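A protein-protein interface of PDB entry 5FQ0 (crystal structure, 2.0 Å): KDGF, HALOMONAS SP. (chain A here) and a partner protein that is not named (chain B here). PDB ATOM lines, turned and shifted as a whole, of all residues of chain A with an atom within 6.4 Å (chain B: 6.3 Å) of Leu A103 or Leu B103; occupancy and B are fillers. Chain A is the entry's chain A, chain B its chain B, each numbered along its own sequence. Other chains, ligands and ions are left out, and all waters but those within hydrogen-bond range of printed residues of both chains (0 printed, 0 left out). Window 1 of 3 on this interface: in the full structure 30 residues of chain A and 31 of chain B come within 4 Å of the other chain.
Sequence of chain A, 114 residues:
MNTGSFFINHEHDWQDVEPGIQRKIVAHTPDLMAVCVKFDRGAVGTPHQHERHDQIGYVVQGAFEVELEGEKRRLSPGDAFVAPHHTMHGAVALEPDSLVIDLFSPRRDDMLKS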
ATOM      1  N   LEU A  32      17.350  12.102   1.771  1.00  0.00           N
ATOM      2  CA  LEU A  32      17.892  13.404   2.122  1.00  0.00           C
ATOM      3  C   LEU A  32      16.857  14.266   2.790  1.00  0.00           C
ATOM      4  O   LEU A  32      15.783  14.478   2.232  1.00  0.00           O
ATOM      5  CB  LEU A  32      18.425  14.111   0.882  1.00  0.00           C
ATOM      6  CG  LEU A  32      19.079  15.471   1.079  1.00  0.00           C
ATOM      7  CD1 LEU A  32      20.364  15.413   1.919  1.00  0.00           C
ATOM      8  CD2 LEU A  32      19.338  16.035  -0.305  1.00  0.00           C
ATOM      9  N   MET A  33      17.204  14.827   3.955  1.00  0.00           N
ATOM     10  CA  MET A  33      16.282  15.691   4.703  1.00  0.00           C
ATOM     11  C   MET A  33      17.006  16.931   5.266  1.00  0.00           C
ATOM     12  O   MET A  33      18.191  16.819   5.654  1.00  0.00           O
ATOM     13  CB  MET A  33      15.661  14.898   5.850  1.00  0.00           C
ATOM     14  CG  MET A  33      14.540  15.637   6.558  1.00  0.00           C
ATOM     15  SD  MET A  33      13.892  14.622   7.885  1.00  0.00           S
ATOM     16  CE  MET A  33      12.129  14.652   7.647  1.00  0.00           C
ATOM     17  N   ALA A  34      16.323  18.093   5.287  1.00  0.00           N
ATOM     18  CA  ALA A  34      16.806  19.324   5.957  1.00  0.00           C
ATOM     19  C   ALA A  34      15.768  19.757   6.945  1.00  0.00           C
ATOM     20  O   ALA A  34      14.567  19.690   6.655  1.00  0.00           O
ATOM     21  CB  ALA A  34      17.108  20.457   4.968  1.00  0.00           C
ATOM     22  N   VAL A  35      16.237  20.184   8.120  1.00  0.00           N
ATOM     23  CA  VAL A  35      15.396  20.615   9.238  1.00  0.00           C
ATOM     24  C   VAL A  35      16.051  21.934   9.723  1.00  0.00           C
ATOM     25  O   VAL A  35      17.276  21.993   9.874  1.00  0.00           O
ATOM     26  CB  VAL A  35      15.403  19.561  10.361  1.00  0.00           C
ATOM     27  CG1 VAL A  35      14.523  19.985  11.549  1.00  0.00           C
ATOM     28  CG2 VAL A  35      14.888  18.214   9.818  1.00  0.00           C
ATOM     29  N   ASP A  54      23.603   9.702   8.643  1.00  0.00           N
ATOM     30  CA  ASP A  54      24.643  10.727   8.665  1.00  0.00           C
ATOM     31  C   ASP A  54      23.976  12.067   8.951  1.00  0.00           C
ATOM     32  O   ASP A  54      22.806  12.256   8.634  1.00  0.00           O
ATOM     33  CB  ASP A  54      25.382  10.791   7.329  1.00  0.00           C
ATOM     34  CG  ASP A  54      26.292   9.589   7.069  1.00  0.00           C
ATOM     35  OD1 ASP A  54      26.816   8.935   8.013  1.00  0.00           O
ATOM     36  OD2 ASP A  54      26.472   9.299   5.861  1.00  0.00           O
ATOM     37  N   GLN A  55      24.722  13.004   9.543  1.00  0.00           N
ATOM     38  CA  GLN A  55      24.174  14.321   9.885  1.00  0.00           C
ATOM     39  C   GLN A  55      25.249  15.365   9.689  1.00  0.00           C
ATOM     40  O   GLN A  55      26.426  15.138  10.030  1.00  0.00           O
ATOM     41  CB  GLN A  55      23.701  14.370  11.363  1.00  0.00           C
ATOM     42  CG  GLN A  55      23.058  15.708  11.737  1.00  0.00           C
ATOM     43  CD  GLN A  55      22.597  15.756  13.194  1.00  0.00           C
ATOM     44  OE1 GLN A  55      22.275  14.712  13.813  1.00  0.00           O
ATOM     45  NE2 GLN A  55      22.520  16.957  13.738  1.00  0.00           N
ATOM     46  N   ILE A  56      24.852  16.489   9.120  1.00  0.00           N
ATOM     47  CA  ILE A  56      25.678  17.694   9.028  1.00  0.00           C
ATOM     48  C   ILE A  56      24.809  18.773   9.674  1.00  0.00           C
ATOM     49  O   ILE A  56      23.558  18.823   9.427  1.00  0.00           O
ATOM     50  CB  ILE A  56      25.984  18.081   7.553  1.00  0.00           C
ATOM     51  CG1 ILE A  56      26.843  16.997   6.857  1.00  0.00           C
ATOM     52  CG2 ILE A  56      26.646  19.475   7.430  1.00  0.00           C
ATOM     53  CD1 ILE A  56      26.937  17.183   5.329  1.00  0.00           C
ATOM     54  N   GLY A  57      25.434  19.596  10.521  1.00  0.00           N
ATOM     55  CA  GLY A  57      24.768  20.751  11.095  1.00  0.00           C
ATOM     56  C   GLY A  57      25.447  21.983  10.526  1.00  0.00           C
ATOM     57  O   GLY A  57      26.665  22.144  10.658  1.00  0.00           O
ATOM     58  N   TYR A  58      24.690  22.845   9.857  1.00  0.00           N
ATOM     59  CA  TYR A  58      25.253  24.068   9.246  1.00  0.00           C
ATOM     60  C   TYR A  58      24.730  25.301   9.999  1.00  0.00           C
ATOM     61  O   TYR A  58      23.518  25.517  10.085  1.00  0.00           O
ATOM     62  CB  TYR A  58      24.868  24.120   7.748  1.00  0.00           C
ATOM     63  CG  TYR A  58      25.399  25.353   7.047  1.00  0.00           C
ATOM     64  CD1 TYR A  58      26.666  25.336   6.463  1.00  0.00           C
ATOM     65  CD2 TYR A  58      24.645  26.536   6.978  1.00  0.00           C
ATOM     66  CE1 TYR A  58      27.188  26.458   5.844  1.00  0.00           C
ATOM     67  CE2 TYR A  58      25.168  27.674   6.361  1.00  0.00           C
ATOM     68  CZ  TYR A  58      26.444  27.608   5.801  1.00  0.00           C
ATOM     69  OH  TYR A  58      26.989  28.673   5.170  1.00  0.00           O
ATOM     70  N   ILE A 101      20.920  24.381  10.513  1.00  0.00           N
ATOM     71  CA  ILE A 101      20.271  23.480   9.571  1.00  0.00           C
ATOM     72  C   ILE A 101      20.855  22.093   9.803  1.00  0.00           C
ATOM     73  O   ILE A 101      22.047  21.878   9.592  1.00  0.00           O
ATOM     74  CB  ILE A 101      20.495  23.904   8.088  1.00  0.00           C
ATOM     75  CG1 ILE A 101      20.094  25.360   7.849  1.00  0.00           C
ATOM     76  CG2 ILE A 101      19.746  22.980   7.137  1.00  0.00           C
ATOM     77  CD1 ILE A 101      18.811  25.804   8.561  1.00  0.00           C
ATOM     78  N   ASP A 102      20.042  21.169  10.301  1.00  0.00           N
ATOM     79  CA  ASP A 102      20.426  19.751  10.396  1.00  0.00           C
ATOM     80  C   ASP A 102      19.995  19.059   9.104  1.00  0.00           C
ATOM     81  O   ASP A 102      18.816  19.131   8.674  1.00  0.00           O
ATOM     82  CB  ASP A 102      19.750  19.078  11.606  1.00  0.00           C
ATOM     83  CG  ASP A 102      20.387  19.474  12.969  1.00  0.00           C
ATOM     84  OD1 ASP A 102      21.586  19.807  13.026  1.00  0.00           O
ATOM     85  OD2 ASP A 102      19.667  19.427  13.978  1.00  0.00           O
ATOM     86  N   LEU A 103      20.962  18.417   8.478  1.00  0.00           N
ATOM     87  CA  LEU A 103      20.788  17.669   7.258  1.00  0.00           C
ATOM     88  C   LEU A 103      21.067  16.223   7.561  1.00  0.00           C
ATOM     89  O   LEU A 103      21.981  15.937   8.321  1.00  0.00           O
ATOM     90  CB  LEU A 103      21.896  18.024   6.346  1.00  0.00           C
ATOM     91  CG  LEU A 103      22.145  19.238   5.557  1.00  0.00           C
ATOM     92  CD1 LEU A 103      22.712  20.375   6.405  1.00  0.00           C
ATOM     93  CD2 LEU A 103      23.205  18.574   4.648  1.00  0.00           C
ATOM     94  N   PHE A 104      20.317  15.316   6.956  1.00  0.00           N
ATOM     95  CA  PHE A 104      20.401  13.895   7.266  1.00  0.00           C
ATOM     96  C   PHE A 104      20.332  13.073   5.975  1.00  0.00           C
ATOM     97  O   PHE A 104      19.679  13.471   4.989  1.00  0.00           O
ATOM     98  CB  PHE A 104      19.222  13.491   8.147  1.00  0.00           C
ATOM     99  CG  PHE A 104      19.195  14.138   9.503  1.00  0.00           C
ATOM    100  CD1 PHE A 104      19.971  13.629  10.546  1.00  0.00           C
ATOM    101  CD2 PHE A 104      18.355  15.228   9.757  1.00  0.00           C
ATOM    102  CE1 PHE A 104      19.910  14.191  11.814  1.00  0.00           C
ATOM    103  CE2 PHE A 104      18.301  15.791  11.018  1.00  0.00           C
ATOM    104  CZ  PHE A 104      19.091  15.276  12.054  1.00  0.00           C
ATOM    105  N   SER A 105      21.042  11.947   5.966  1.00  0.00           N
ATOM    106  CA  SER A 105      20.840  10.907   4.972  1.00  0.00           C
ATOM    107  C   SER A 105      20.921   9.577   5.707  1.00  0.00           C
ATOM    108  O   SER A 105      21.875   9.366   6.465  1.00  0.00           O
ATOM    109  CB  SER A 105      21.910  10.930   3.907  1.00  0.00           C
ATOM    110  OG  SER A 105      21.588   9.901   2.985  1.00  0.00           O
ATOM    111  N   LEU B  32      26.313  11.961   2.081  1.00  0.00           N
ATOM    112  CA  LEU B  32      25.776  13.283   2.386  1.00  0.00           C
ATOM    113  C   LEU B  32      26.843  14.334   2.190  1.00  0.00           C
ATOM    114  O   LEU B  32      27.979  14.148   2.589  1.00  0.00           O
ATOM    115  CB  LEU B  32      25.292  13.325   3.850  1.00  0.00           C
ATOM    116  CG  LEU B  32      24.491  14.526   4.354  1.00  0.00           C
ATOM    117  CD1 LEU B  32      23.241  14.729   3.515  1.00  0.00           C
ATOM    118  CD2 LEU B  32      24.159  14.364   5.839  1.00  0.00           C
ATOM    119  N   MET B  33      26.466  15.458   1.588  1.00  0.00           N
ATOM    120  CA  MET B  33      27.418  16.518   1.305  1.00  0.00           C
ATOM    121  C   MET B  33      26.718  17.884   1.356  1.00  0.00           C
ATOM    122  O   MET B  33      25.540  18.008   0.958  1.00  0.00           O
ATOM    123  CB  MET B  33      28.039  16.284  -0.080  1.00  0.00           C
ATOM    124  CG  MET B  33      28.999  17.378  -0.566  1.00  0.00           C
ATOM    125  SD  MET B  33      29.732  17.069  -2.198  1.00  0.00           S
ATOM    126  CE  MET B  33      31.445  16.766  -1.863  1.00  0.00           C
ATOM    127  N   ALA B  34      27.441  18.888   1.843  1.00  0.00           N
ATOM    128  CA  ALA B  34      26.981  20.269   1.848  1.00  0.00           C
ATOM    129  C   ALA B  34      28.040  21.116   1.151  1.00  0.00           C
ATOM    130  O   ALA B  34      29.239  20.940   1.394  1.00  0.00           O
ATOM    131  CB  ALA B  34      26.745  20.765   3.290  1.00  0.00           C
ATOM    132  N   VAL B  35      27.591  22.040   0.305  1.00  0.00           N
ATOM    133  CA  VAL B  35      28.471  22.927  -0.446  1.00  0.00           C
ATOM    134  C   VAL B  35      27.901  24.328  -0.283  1.00  0.00           C
ATOM    135  O   VAL B  35      26.698  24.526  -0.427  1.00  0.00           O
ATOM    136  CB  VAL B  35      28.493  22.566  -1.958  1.00  0.00           C
ATOM    137  CG1 VAL B  35      29.502  23.430  -2.702  1.00  0.00           C
ATOM    138  CG2 VAL B  35      28.789  21.077  -2.166  1.00  0.00           C
ATOM    139  N   ASP B  54      19.962  13.282  -5.100  1.00  0.00           N
ATOM    140  CA  ASP B  54      18.910  14.198  -4.637  1.00  0.00           C
ATOM    141  C   ASP B  54      19.630  15.490  -4.235  1.00  0.00           C
ATOM    142  O   ASP B  54      20.798  15.454  -3.839  1.00  0.00           O
ATOM    143  CB  ASP B  54      18.148  13.659  -3.406  1.00  0.00           C
ATOM    144  CG  ASP B  54      17.353  12.380  -3.695  1.00  0.00           C
ATOM    145  OD1 ASP B  54      16.870  12.212  -4.844  1.00  0.00           O
ATOM    146  OD2 ASP B  54      17.133  11.589  -2.753  1.00  0.00           O
ATOM    147  N   GLN B  55      18.945  16.621  -4.369  1.00  0.00           N
ATOM    148  CA  GLN B  55      19.506  17.921  -4.063  1.00  0.00           C
ATOM    149  C   GLN B  55      18.501  18.750  -3.279  1.00  0.00           C
ATOM    150  O   GLN B  55      17.296  18.765  -3.599  1.00  0.00           O
ATOM    151  CB  GLN B  55      19.913  18.682  -5.315  1.00  0.00           C
ATOM    152  CG  GLN B  55      20.650  19.979  -4.938  1.00  0.00           C
ATOM    153  CD  GLN B  55      21.101  20.734  -6.144  1.00  0.00           C
ATOM    154  OE1 GLN B  55      21.319  20.129  -7.180  1.00  0.00           O
ATOM    155  NE2 GLN B  55      21.248  22.075  -6.030  1.00  0.00           N
ATOM    156  N   ILE B  56      18.986  19.417  -2.231  1.00  0.00           N
ATOM    157  CA  ILE B  56      18.243  20.506  -1.609  1.00  0.00           C
ATOM    158  C   ILE B  56      19.085  21.770  -1.732  1.00  0.00           C
ATOM    159  O   ILE B  56      20.305  21.739  -1.483  1.00  0.00           O
ATOM    160  CB  ILE B  56      17.867  20.192  -0.121  1.00  0.00           C
ATOM    161  CG1 ILE B  56      16.790  19.079  -0.065  1.00  0.00           C
ATOM    162  CG2 ILE B  56      17.325  21.446   0.604  1.00  0.00           C
ATOM    163  CD1 ILE B  56      16.561  18.512   1.311  1.00  0.00           C
ATOM    164  N   GLY B  57      18.457  22.885  -2.105  1.00  0.00           N
ATOM    165  CA  GLY B  57      19.121  24.200  -2.046  1.00  0.00           C
ATOM    166  C   GLY B  57      18.493  25.052  -0.957  1.00  0.00           C
ATOM    167  O   GLY B  57      17.298  25.389  -0.996  1.00  0.00           O
ATOM    168  N   TYR B  58      19.269  25.363   0.069  1.00  0.00           N
ATOM    169  CA  TYR B  58      18.783  26.189   1.148  1.00  0.00           C
ATOM    170  C   TYR B  58      19.416  27.593   1.045  1.00  0.00           C
ATOM    171  O   TYR B  58      20.661  27.721   1.041  1.00  0.00           O
ATOM    172  CB  TYR B  58      19.151  25.533   2.473  1.00  0.00           C
ATOM    173  CG  TYR B  58      18.612  26.309   3.660  1.00  0.00           C
ATOM    174  CD1 TYR B  58      19.351  27.357   4.235  1.00  0.00           C
ATOM    175  CD2 TYR B  58      17.366  26.014   4.186  1.00  0.00           C
ATOM    176  CE1 TYR B  58      18.856  28.071   5.312  1.00  0.00           C
ATOM    177  CE2 TYR B  58      16.877  26.697   5.276  1.00  0.00           C
ATOM    178  CZ  TYR B  58      17.618  27.726   5.820  1.00  0.00           C
ATOM    179  OH  TYR B  58      17.106  28.423   6.877  1.00  0.00           O
ATOM    180  N   ILE B 101      23.146  27.011   0.134  1.00  0.00           N
ATOM    181  CA  ILE B 101      23.791  25.772   0.562  1.00  0.00           C
ATOM    182  C   ILE B 101      23.164  24.673  -0.287  1.00  0.00           C
ATOM    183  O   ILE B 101      21.951  24.392  -0.139  1.00  0.00           O
ATOM    184  CB  ILE B 101      23.570  25.500   2.074  1.00  0.00           C
ATOM    185  CG1 ILE B 101      23.844  26.738   2.907  1.00  0.00           C
ATOM    186  CG2 ILE B 101      24.521  24.418   2.547  1.00  0.00           C
ATOM    187  CD1 ILE B 101      25.214  27.354   2.668  1.00  0.00           C
ATOM    188  N   ASP B 102      23.940  24.103  -1.212  1.00  0.00           N
ATOM    189  CA  ASP B 102      23.463  22.931  -1.933  1.00  0.00           C
ATOM    190  C   ASP B 102      23.785  21.682  -1.118  1.00  0.00           C
ATOM    191  O   ASP B 102      24.943  21.472  -0.743  1.00  0.00           O
ATOM    192  CB  ASP B 102      24.109  22.819  -3.312  1.00  0.00           C
ATOM    193  CG  ASP B 102      23.527  23.793  -4.299  1.00  0.00           C
ATOM    194  OD1 ASP B 102      22.326  24.133  -4.174  1.00  0.00           O
ATOM    195  OD2 ASP B 102      24.279  24.169  -5.210  1.00  0.00           O
ATOM    196  N   LEU B 103      22.753  20.872  -0.860  1.00  0.00           N
ATOM    197  CA  LEU B 103      22.855  19.624  -0.090  1.00  0.00           C
ATOM    198  C   LEU B 103      22.572  18.434  -1.014  1.00  0.00           C
ATOM    199  O   LEU B 103      21.632  18.487  -1.806  1.00  0.00           O
ATOM    200  CB  LEU B 103      21.836  19.650   1.063  1.00  0.00           C
ATOM    201  CG  LEU B 103      21.732  21.075   1.638  1.00  0.00           C
ATOM    202  CD1 LEU B 103      20.501  21.218   2.491  1.00  0.00           C
ATOM    203  CD2 LEU B 103      22.991  21.407   2.442  1.00  0.00           C
ATOM    204  N   PHE B 104      23.361  17.370  -0.895  1.00  0.00           N
ATOM    205  CA  PHE B 104      23.271  16.232  -1.822  1.00  0.00           C
ATOM    206  C   PHE B 104      23.282  14.899  -1.087  1.00  0.00           C
ATOM    207  O   PHE B 104      23.891  14.774  -0.025  1.00  0.00           O
ATOM    208  CB  PHE B 104      24.439  16.214  -2.833  1.00  0.00           C
ATOM    209  CG  PHE B 104      24.502  17.420  -3.750  1.00  0.00           C
ATOM    210  CD1 PHE B 104      23.777  17.454  -4.945  1.00  0.00           C
ATOM    211  CD2 PHE B 104      25.316  18.509  -3.422  1.00  0.00           C
ATOM    212  CE1 PHE B 104      23.874  18.545  -5.798  1.00  0.00           C
ATOM    213  CE2 PHE B 104      25.410  19.611  -4.243  1.00  0.00           C
ATOM    214  CZ  PHE B 104      24.684  19.638  -5.445  1.00  0.00           C
ATOM    215  N   SER B 105      22.597  13.908  -1.661  1.00  0.00           N
ATOM    216  CA  SER B 105      22.756  12.516  -1.273  1.00  0.00           C
ATOM    217  C   SER B 105      22.682  11.713  -2.577  1.00  0.00           C
ATOM    218  O   SER B 105      21.748  11.914  -3.359  1.00  0.00           O
ATOM    219  CB  SER B 105      21.661  12.068  -0.322  1.00  0.00           C
ATOM    220  OG  SER B 105      21.868  10.694   0.019  1.00  0.00           O
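The side-chain hydroxyl (OG) of Ser A105 lies within hydrogen-bond range of the side-chain hydroxyl (OG) of Ser B105 (3.1 Å).
The backbone carbonyl oxygen (O) of Ile A56 lies within hydrogen-bond range of the backbone NH (N) of Leu A103 (2.8 Å).
The side-chain amide nitrogen (NE2) of Gln A55 is in hydrogen-bond range of the side-chain carboxylate (OD1) of Asp A102, at 3.1 Å.
O of Tyr B58 is in hydrogen-bond range of N of Ile B101 (2.7 Å).
The backbone NH (N) of Tyr A58 lies within hydrogen-bond range of the backbone carbonyl oxygen (O) of Ile A101 (2.8 Å).
N of Asp A54 sits at hydrogen-bond distance from O of Ser A105 (2.8 Å).
N of Asp B54 lies within hydrogen-bond range of O of Ser B105 (2.8 Å).
Leu B32 touches Leu A32.
Asp B54 touches Leu A32.
Leu A32 touches Ile B56 (CD2 to N, 3.9 Å).
Asp A54 touches Leu B32 (O to CD2, 3.8 Å).
Leu B32 touches Gln A55 (CD2 to N, 3.99 Å).
Ile A56 touches Leu B32 (CD1 to CG, 3.7 Å).
CD1 of Ile A56 touches N of Ala B34, 3.9 Å away.
Tyr A58 touches Ile B101 (OH to CD1, 3.3 Å).
Leu A103 touches Leu B32 (O to CD2, 3.7 Å).
Leu B103 touches Leu A103.
Of the printed residues of chain B, Asp A54 touches Leu B32 (3.8 Å).
Printed residues of chain A within 4 Å of Leu B32: Leu A32, Asp A54, Gln A55, Ile A56, Leu A103 and Ser A105.
Gly B57 touches none of the printed residues of chain A.
Printed residues of chain A within 4 Å of Tyr B58: Ile A101.
Of chain A, only Leu A32 and Leu A103 come within 4 Å of Leu B103.
The nearest printed residue of chain B that does not touch Leu A103 is Ala B34 (4.4 Å).
The nearest residue of chain A that does not touch Leu B103 is Ala A34 (4.3 Å).
The nearest printed residue of chain A that does not touch Ile B56 is Ala A34 (4.01 Å).
Hydrophobic or aromatic side chains of chain B within 4 Å of the printed part of chain A: Leu B32, Ile B56, Tyr B58, Ile B101 and Leu B103.
Of the 14 printed residues of chain A, 8 touch a printed residue of chain B.
Among the printed residues, 14 pairs touch across the chains.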
